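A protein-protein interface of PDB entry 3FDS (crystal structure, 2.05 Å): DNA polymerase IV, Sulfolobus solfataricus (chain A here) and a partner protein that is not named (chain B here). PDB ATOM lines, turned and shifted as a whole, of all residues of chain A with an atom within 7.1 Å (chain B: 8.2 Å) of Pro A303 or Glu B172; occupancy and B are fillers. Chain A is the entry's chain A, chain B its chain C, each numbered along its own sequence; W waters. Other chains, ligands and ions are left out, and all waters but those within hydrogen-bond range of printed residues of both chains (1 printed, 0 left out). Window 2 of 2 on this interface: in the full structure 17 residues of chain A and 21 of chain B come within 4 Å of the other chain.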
ATOM      1  N   PRO A 281      18.341  17.023  20.421  1.00  0.00           N
ATOM      2  CA  PRO A 281      19.615  16.785  19.761  1.00  0.00           C
ATOM      3  C   PRO A 281      20.745  17.375  20.567  1.00  0.00           C
ATOM      4  O   PRO A 281      20.559  18.419  21.199  1.00  0.00           O
ATOM      5  CB  PRO A 281      19.495  17.562  18.446  1.00  0.00           C
ATOM      6  CG  PRO A 281      18.435  18.636  18.705  1.00  0.00           C
ATOM      7  CD  PRO A 281      17.588  18.146  19.818  1.00  0.00           C
ATOM      8  N   LYS A 282      21.902  16.730  20.515  1.00  0.00           N
ATOM      9  CA  LYS A 282      23.105  17.267  21.140  1.00  0.00           C
ATOM     10  C   LYS A 282      23.967  18.020  20.186  1.00  0.00           C
ATOM     11  O   LYS A 282      24.801  18.811  20.632  1.00  0.00           O
ATOM     12  CB  LYS A 282      23.942  16.199  21.822  1.00  0.00           C
ATOM     13  CG  LYS A 282      23.241  15.539  23.026  1.00  0.00           C
ATOM     14  CD  LYS A 282      23.883  14.203  23.366  1.00  0.00           C
ATOM     15  CE  LYS A 282      25.302  14.358  23.905  1.00  0.00           C
ATOM     16  NZ  LYS A 282      25.399  14.171  25.385  1.00  0.00           N
ATOM     17  N   THR A 301      28.501  20.823  19.365  1.00  0.00           N
ATOM     18  CA  THR A 301      27.874  19.823  20.212  1.00  0.00           C
ATOM     19  C   THR A 301      27.662  20.432  21.622  1.00  0.00           C
ATOM     20  O   THR A 301      28.501  21.171  22.113  1.00  0.00           O
ATOM     21  CB  THR A 301      28.733  18.557  20.229  1.00  0.00           C
ATOM     22  OG1 THR A 301      28.733  17.989  18.908  1.00  0.00           O
ATOM     23  CG2 THR A 301      28.199  17.482  21.216  1.00  0.00           C
ATOM     24  N   PHE A 302      26.500  20.176  22.212  1.00  0.00           N
ATOM     25  CA  PHE A 302      26.170  20.646  23.542  1.00  0.00           C
ATOM     26  C   PHE A 302      25.822  19.404  24.334  1.00  0.00           C
ATOM     27  O   PHE A 302      24.802  18.787  24.062  1.00  0.00           O
ATOM     28  CB  PHE A 302      24.953  21.551  23.473  1.00  0.00           C
ATOM     29  CG  PHE A 302      25.206  22.843  22.779  1.00  0.00           C
ATOM     30  CD1 PHE A 302      25.184  22.915  21.380  1.00  0.00           C
ATOM     31  CD2 PHE A 302      25.435  23.993  23.523  1.00  0.00           C
ATOM     32  CE1 PHE A 302      25.419  24.142  20.724  1.00  0.00           C
ATOM     33  CE2 PHE A 302      25.655  25.214  22.898  1.00  0.00           C
ATOM     34  CZ  PHE A 302      25.659  25.295  21.500  1.00  0.00           C
ATOM     35  N   PRO A 303      26.660  19.039  25.313  1.00  0.00           N
ATOM     36  CA  PRO A 303      26.451  17.777  26.042  1.00  0.00           C
ATOM     37  C   PRO A 303      25.027  17.608  26.592  1.00  0.00           C
ATOM     38  O   PRO A 303      24.500  16.485  26.596  1.00  0.00           O
ATOM     39  CB  PRO A 303      27.492  17.826  27.145  1.00  0.00           C
ATOM     40  CG  PRO A 303      28.601  18.614  26.571  1.00  0.00           C
ATOM     41  CD  PRO A 303      27.962  19.648  25.637  1.00  0.00           C
ATOM     42  N   HIS A 304      24.389  18.700  27.017  1.00  0.00           N
ATOM     43  CA  HIS A 304      23.001  18.614  27.451  1.00  0.00           C
ATOM     44  C   HIS A 304      22.158  18.952  26.214  1.00  0.00           C
ATOM     45  O   HIS A 304      22.667  19.184  25.099  1.00  0.00           O
ATOM     46  CB  HIS A 304      22.767  19.429  28.755  1.00  0.00           C
ATOM     47  CG  HIS A 304      23.492  18.859  29.948  1.00  0.00           C
ATOM     48  ND1 HIS A 304      22.892  18.005  30.848  1.00  0.00           N
ATOM     49  CD2 HIS A 304      24.777  18.989  30.363  1.00  0.00           C
ATOM     50  CE1 HIS A 304      23.771  17.628  31.762  1.00  0.00           C
ATOM     51  NE2 HIS A 304      24.925  18.209  31.486  1.00  0.00           N
ATOM     52  N   GLY A 305      20.855  18.916  26.245  1.00  0.00           N
ATOM     53  CA  GLY A 305      20.309  19.081  24.836  1.00  0.00           C
ATOM     54  C   GLY A 305      20.512  20.447  24.143  1.00  0.00           C
ATOM     55  O   GLY A 305      21.098  21.386  24.710  1.00  0.00           O
ATOM     56  N   ILE A 306      20.020  20.560  22.906  1.00  0.00           N
ATOM     57  CA  ILE A 306      19.807  21.863  22.261  1.00  0.00           C
ATOM     58  C   ILE A 306      18.302  22.145  22.160  1.00  0.00           C
ATOM     59  O   ILE A 306      17.629  21.505  21.366  1.00  0.00           O
ATOM     60  CB  ILE A 306      20.414  21.896  20.819  1.00  0.00           C
ATOM     61  CG1 ILE A 306      21.877  21.468  20.861  1.00  0.00           C
ATOM     62  CG2 ILE A 306      20.264  23.277  20.147  1.00  0.00           C
ATOM     63  CD1 ILE A 306      22.417  21.220  19.430  1.00  0.00           C
ATOM     64  N   ILE A 341      19.021  12.603  22.269  1.00  0.00           N
ATOM     65  CA  ILE A 341      18.708  12.045  23.583  1.00  0.00           C
ATOM     66  C   ILE A 341      17.232  11.652  23.485  1.00  0.00           C
ATOM     67  O   ILE A 341      16.366  12.520  23.253  1.00  0.00           O
ATOM     68  CB  ILE A 341      18.898  13.116  24.700  1.00  0.00           C
ATOM     69  CG1 ILE A 341      20.381  13.559  24.772  1.00  0.00           C
ATOM     70  CG2 ILE A 341      18.336  12.613  26.054  1.00  0.00           C
ATOM     71  CD1 ILE A 341      20.636  14.824  25.607  1.00  0.00           C
ATOM     72  N   VAL B 150      29.767  11.078  37.651  1.00  0.00           N
ATOM     73  CA  VAL B 150      29.105  10.946  36.347  1.00  0.00           C
ATOM     74  C   VAL B 150      28.598  12.273  35.843  1.00  0.00           C
ATOM     75  O   VAL B 150      28.718  12.616  34.646  1.00  0.00           O
ATOM     76  CB  VAL B 150      28.016   9.830  36.258  1.00  0.00           C
ATOM     77  CG1 VAL B 150      28.658   8.451  36.509  1.00  0.00           C
ATOM     78  CG2 VAL B 150      26.782  10.051  37.152  1.00  0.00           C
ATOM     79  N   THR B 151      28.096  13.057  36.784  1.00  0.00           N
ATOM     80  CA  THR B 151      27.408  14.250  36.478  1.00  0.00           C
ATOM     81  C   THR B 151      28.459  15.322  36.039  1.00  0.00           C
ATOM     82  O   THR B 151      28.192  16.168  35.211  1.00  0.00           O
ATOM     83  CB  THR B 151      26.525  14.468  37.753  1.00  0.00           C
ATOM     84  OG1 THR B 151      25.112  14.349  37.471  1.00  0.00           O
ATOM     85  CG2 THR B 151      26.991  15.564  38.573  1.00  0.00           C
ATOM     86  N   LEU B 152      29.669  15.237  36.587  1.00  0.00           N
ATOM     87  CA  LEU B 152      30.778  16.098  36.142  1.00  0.00           C
ATOM     88  C   LEU B 152      31.150  15.821  34.648  1.00  0.00           C
ATOM     89  O   LEU B 152      31.596  16.703  33.906  1.00  0.00           O
ATOM     90  CB  LEU B 152      32.057  15.743  36.957  1.00  0.00           C
ATOM     91  CG  LEU B 152      33.326  16.490  36.595  1.00  0.00           C
ATOM     92  CD1 LEU B 152      33.117  17.981  36.990  1.00  0.00           C
ATOM     93  CD2 LEU B 152      34.659  15.887  37.161  1.00  0.00           C
ATOM     94  N   VAL B 153      31.016  14.566  34.242  1.00  0.00           N
ATOM     95  CA  VAL B 153      31.581  14.133  32.954  1.00  0.00           C
ATOM     96  C   VAL B 153      30.526  14.006  31.820  1.00  0.00           C
ATOM     97  O   VAL B 153      30.818  14.258  30.669  1.00  0.00           O
ATOM     98  CB  VAL B 153      32.311  12.770  33.205  1.00  0.00           C
ATOM     99  CG1 VAL B 153      32.565  12.077  31.940  1.00  0.00           C
ATOM    100  CG2 VAL B 153      33.671  13.061  34.001  1.00  0.00           C
ATOM    101  N   GLY B 154      29.314  13.556  32.127  1.00  0.00           N
ATOM    102  CA  GLY B 154      28.325  13.399  31.038  1.00  0.00           C
ATOM    103  C   GLY B 154      26.864  13.505  31.448  1.00  0.00           C
ATOM    104  O   GLY B 154      26.533  13.589  32.627  1.00  0.00           O
ATOM    105  N   GLU B 155      25.998  13.556  30.441  1.00  0.00           N
ATOM    106  CA  GLU B 155      24.561  13.784  30.616  1.00  0.00           C
ATOM    107  C   GLU B 155      23.996  12.372  30.861  1.00  0.00           C
ATOM    108  O   GLU B 155      22.917  12.213  31.382  1.00  0.00           O
ATOM    109  CB  GLU B 155      24.058  14.373  29.266  1.00  0.00           C
ATOM    110  CG  GLU B 155      22.607  14.744  29.158  1.00  0.00           C
ATOM    111  CD  GLU B 155      21.701  13.555  28.896  1.00  0.00           C
ATOM    112  OE1 GLU B 155      20.558  13.595  29.369  1.00  0.00           O
ATOM    113  OE2 GLU B 155      22.139  12.568  28.234  1.00  0.00           O
ATOM    114  N   GLU B 156      24.708  11.347  30.378  1.00  0.00           N
ATOM    115  CA  GLU B 156      24.155   9.985  30.410  1.00  0.00           C
ATOM    116  C   GLU B 156      25.182   9.041  31.056  1.00  0.00           C
ATOM    117  O   GLU B 156      26.390   9.231  30.902  1.00  0.00           O
ATOM    118  CB  GLU B 156      23.796   9.516  28.979  1.00  0.00           C
ATOM    119  CG  GLU B 156      23.245   8.102  28.866  1.00  0.00           C
ATOM    120  CD  GLU B 156      22.922   7.735  27.406  1.00  0.00           C
ATOM    121  OE1 GLU B 156      23.757   7.142  26.724  1.00  0.00           O
ATOM    122  OE2 GLU B 156      21.838   8.060  26.921  1.00  0.00           O
ATOM    123  N   MET B 157      24.709   8.057  31.819  1.00  0.00           N
ATOM    124  CA  MET B 157      25.639   7.105  32.376  1.00  0.00           C
ATOM    125  C   MET B 157      25.252   5.718  31.898  1.00  0.00           C
ATOM    126  O   MET B 157      24.077   5.461  31.645  1.00  0.00           O
ATOM    127  CB  MET B 157      25.627   7.165  33.924  1.00  0.00           C
ATOM    128  CG  MET B 157      24.346   6.630  34.491  1.00  0.00           C
ATOM    129  SD  MET B 157      24.117   6.901  36.252  1.00  0.00           S
ATOM    130  CE  MET B 157      25.357   5.782  36.977  1.00  0.00           C
ATOM    131  N   ALA B 170      30.630   7.098  31.838  1.00  0.00           N
ATOM    132  CA  ALA B 170      29.941   8.316  31.365  1.00  0.00           C
ATOM    133  C   ALA B 170      30.951   9.020  30.521  1.00  0.00           C
ATOM    134  O   ALA B 170      32.139   8.785  30.668  1.00  0.00           O
ATOM    135  CB  ALA B 170      29.558   9.183  32.549  1.00  0.00           C
ATOM    136  N   GLY B 171      30.499   9.873  29.601  1.00  0.00           N
ATOM    137  CA  GLY B 171      31.419  10.647  28.832  1.00  0.00           C
ATOM    138  C   GLY B 171      30.807  11.471  27.729  1.00  0.00           C
ATOM    139  O   GLY B 171      29.688  11.260  27.305  1.00  0.00           O
ATOM    140  N   GLU B 172      31.581  12.424  27.246  1.00  0.00           N
ATOM    141  CA  GLU B 172      31.162  13.263  26.153  1.00  0.00           C
ATOM    142  C   GLU B 172      32.398  13.360  25.303  1.00  0.00           C
ATOM    143  O   GLU B 172      33.428  13.841  25.782  1.00  0.00           O
ATOM    144  CB  GLU B 172      30.742  14.654  26.677  1.00  0.00           C
ATOM    145  CG  GLU B 172      29.571  14.662  27.659  1.00  0.00           C
ATOM    146  CD  GLU B 172      28.230  14.214  27.056  1.00  0.00           C
ATOM    147  OE1 GLU B 172      28.136  14.086  25.802  1.00  0.00           O
ATOM    148  OE2 GLU B 172      27.252  14.002  27.835  1.00  0.00           O
ATOM    149  N   GLU B 173      32.294  12.895  24.056  1.00  0.00           N
ATOM    150  CA  GLU B 173      33.371  12.950  23.080  1.00  0.00           C
ATOM    151  C   GLU B 173      34.683  12.420  23.719  1.00  0.00           C
ATOM    152  O   GLU B 173      34.697  11.353  24.387  1.00  0.00           O
ATOM    153  CB  GLU B 173      33.458  14.366  22.509  1.00  0.00           C
ATOM    154  CG  GLU B 173      32.068  14.890  22.066  1.00  0.00           C
ATOM    155  CD  GLU B 173      32.187  16.007  21.011  1.00  0.00           C
ATOM    156  OE1 GLU B 173      32.416  17.186  21.384  1.00  0.00           O
ATOM    157  OE2 GLU B 173      32.050  15.709  19.811  1.00  0.00           O
ATOM    158  N   GLY B 174      35.806  13.063  23.609  1.00  0.00           N
ATOM    159  CA  GLY B 174      36.895  12.280  24.323  1.00  0.00           C
ATOM    160  C   GLY B 174      36.811  12.016  25.856  1.00  0.00           C
ATOM    161  O   GLY B 174      37.507  11.142  26.422  1.00  0.00           O
ATOM    162  N   LYS B 175      35.973  12.785  26.537  1.00  0.00           N
ATOM    163  CA  LYS B 175      36.164  13.045  27.976  1.00  0.00           C
ATOM    164  C   LYS B 175      35.303  12.136  28.812  1.00  0.00           C
ATOM    165  O   LYS B 175      34.107  12.379  28.923  1.00  0.00           O
ATOM    166  CB  LYS B 175      35.830  14.521  28.309  1.00  0.00           C
ATOM    167  CG  LYS B 175      36.681  15.572  27.537  1.00  0.00           C
ATOM    168  CD  LYS B 175      36.430  16.952  28.087  1.00  0.00           C
ATOM    169  CE  LYS B 175      36.893  18.015  27.132  1.00  0.00           C
ATOM    170  NZ  LYS B 175      36.777  19.381  27.703  1.00  0.00           N
ATOM    171  N   ARG B 176      35.914  11.157  29.478  1.00  0.00           N
ATOM    172  CA  ARG B 176      35.215   9.978  29.924  1.00  0.00           C
ATOM    173  C   ARG B 176      35.544   9.703  31.367  1.00  0.00           C
ATOM    174  O   ARG B 176      36.539  10.211  31.906  1.00  0.00           O
ATOM    175  CB  ARG B 176      35.670   8.734  29.116  1.00  0.00           C
ATOM    176  CG  ARG B 176      34.837   8.478  27.872  1.00  0.00           C
ATOM    177  CD  ARG B 176      35.426   7.367  27.000  1.00  0.00           C
ATOM    178  NE  ARG B 176      35.785   6.132  27.719  1.00  0.00           N
ATOM    179  CZ  ARG B 176      34.926   5.202  28.177  1.00  0.00           C
ATOM    180  NH1 ARG B 176      33.597   5.343  28.044  1.00  0.00           N
ATOM    181  NH2 ARG B 176      35.403   4.115  28.785  1.00  0.00           N
ATOM    182  N   TYR B 177      34.702   8.879  31.971  1.00  0.00           N
ATOM    183  CA  TYR B 177      34.844   8.398  33.327  1.00  0.00           C
ATOM    184  C   TYR B 177      34.529   6.918  33.300  1.00  0.00           C
ATOM    185  O   TYR B 177      33.586   6.511  32.603  1.00  0.00           O
ATOM    186  CB  TYR B 177      33.730   9.022  34.191  1.00  0.00           C
ATOM    187  CG  TYR B 177      33.562   8.459  35.590  1.00  0.00           C
ATOM    188  CD1 TYR B 177      34.494   8.715  36.588  1.00  0.00           C
ATOM    189  CD2 TYR B 177      32.423   7.708  35.924  1.00  0.00           C
ATOM    190  CE1 TYR B 177      34.309   8.207  37.881  1.00  0.00           C
ATOM    191  CE2 TYR B 177      32.227   7.219  37.172  1.00  0.00           C
ATOM    192  CZ  TYR B 177      33.150   7.494  38.171  1.00  0.00           C
ATOM    193  OH  TYR B 177      32.908   7.053  39.458  1.00  0.00           O
ATOM    194  N   ALA B 202      22.024  10.757  33.884  1.00  0.00           N
ATOM    195  CA  ALA B 202      22.863  10.985  35.043  1.00  0.00           C
ATOM    196  C   ALA B 202      22.166  11.923  36.062  1.00  0.00           C
ATOM    197  O   ALA B 202      22.325  11.721  37.245  1.00  0.00           O
ATOM    198  CB  ALA B 202      24.208  11.560  34.618  1.00  0.00           C
ATOM    199  N   ARG B 248      17.623   4.591  28.799  1.00  0.00           N
ATOM    200  CA  ARG B 248      17.775   5.150  27.436  1.00  0.00           C
ATOM    201  C   ARG B 248      17.826   3.983  26.460  1.00  0.00           C
ATOM    202  O   ARG B 248      18.633   3.039  26.598  1.00  0.00           O
ATOM    203  CB  ARG B 248      19.079   5.956  27.328  1.00  0.00           C
ATOM    204  CG  ARG B 248      19.136   7.172  28.293  1.00  0.00           C
ATOM    205  CD  ARG B 248      18.485   8.340  27.632  1.00  0.00           C
ATOM    206  NE  ARG B 248      18.246   9.505  28.481  1.00  0.00           N
ATOM    207  CZ  ARG B 248      19.139  10.439  28.767  1.00  0.00           C
ATOM    208  NH1 ARG B 248      20.396  10.327  28.318  1.00  0.00           N
ATOM    209  NH2 ARG B 248      18.771  11.488  29.527  1.00  0.00           N
HETATM  210  O   HOH W   1      23.891  12.045  26.352  1.00  0.00           O
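Water W1 lies within hydrogen-bond range of OE2 of Glu B155 and NZ of Lys A282.
OE1 of Glu B172 is in salt-bridge range of NZ of Lys A282.
Among the printed residues, merely in contact across the chains: Pro A303 with Glu B155, Ile A341 with Arg B248, Ile A341 with Glu B155, His A304 with Glu B155 and Pro A303 with Glu B172.
Among the printed residues, 6 pairs touch across the chains.
Printed residues of chain B within 4 Å of Pro A303: Glu B155 (3.4 Å) and Glu B172 (3.7 Å). Glu B172 touches just these residues of chain A: Lys A282 (2.8 Å) and Pro A303 (3.7 Å). Of the printed residues of chain B, Ile A341 touches Glu B155 and Arg B248. Of the printed residues of chain A, Glu B155 touches Pro A303 (3.4 Å), His A304 (3.7 Å) and Ile A341 (3.7 Å). The nearest printed residue of chain A that does not touch Arg B248 is Lys A282 (7.0 Å).
The backbone carbonyl oxygen (O) of Lys A282 sits at hydrogen-bond distance from the backbone NH (N) of Phe A302. The side-chain amino group (NZ) of Lys A282 sits at hydrogen-bond distance from the backbone carbonyl oxygen (O) of Pro A303, 2.8 Å away. N of Glu B155 lies within hydrogen-bond range of OE2 of Glu B172 (2.9 Å). The backbone carbonyl oxygen of Glu B155 lies within hydrogen-bond range of the backbone NH of Ala B202 (3.0 Å). The side-chain carboxylate (OE1) of Glu B155 lies within salt-bridge range of the guanidinium group (NH2) of Arg B248 (2.8 Å). The guanidinium group (NH1) of Arg B248 is in salt-bridge range of the side-chain carboxylate (OE2) of Glu B156.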
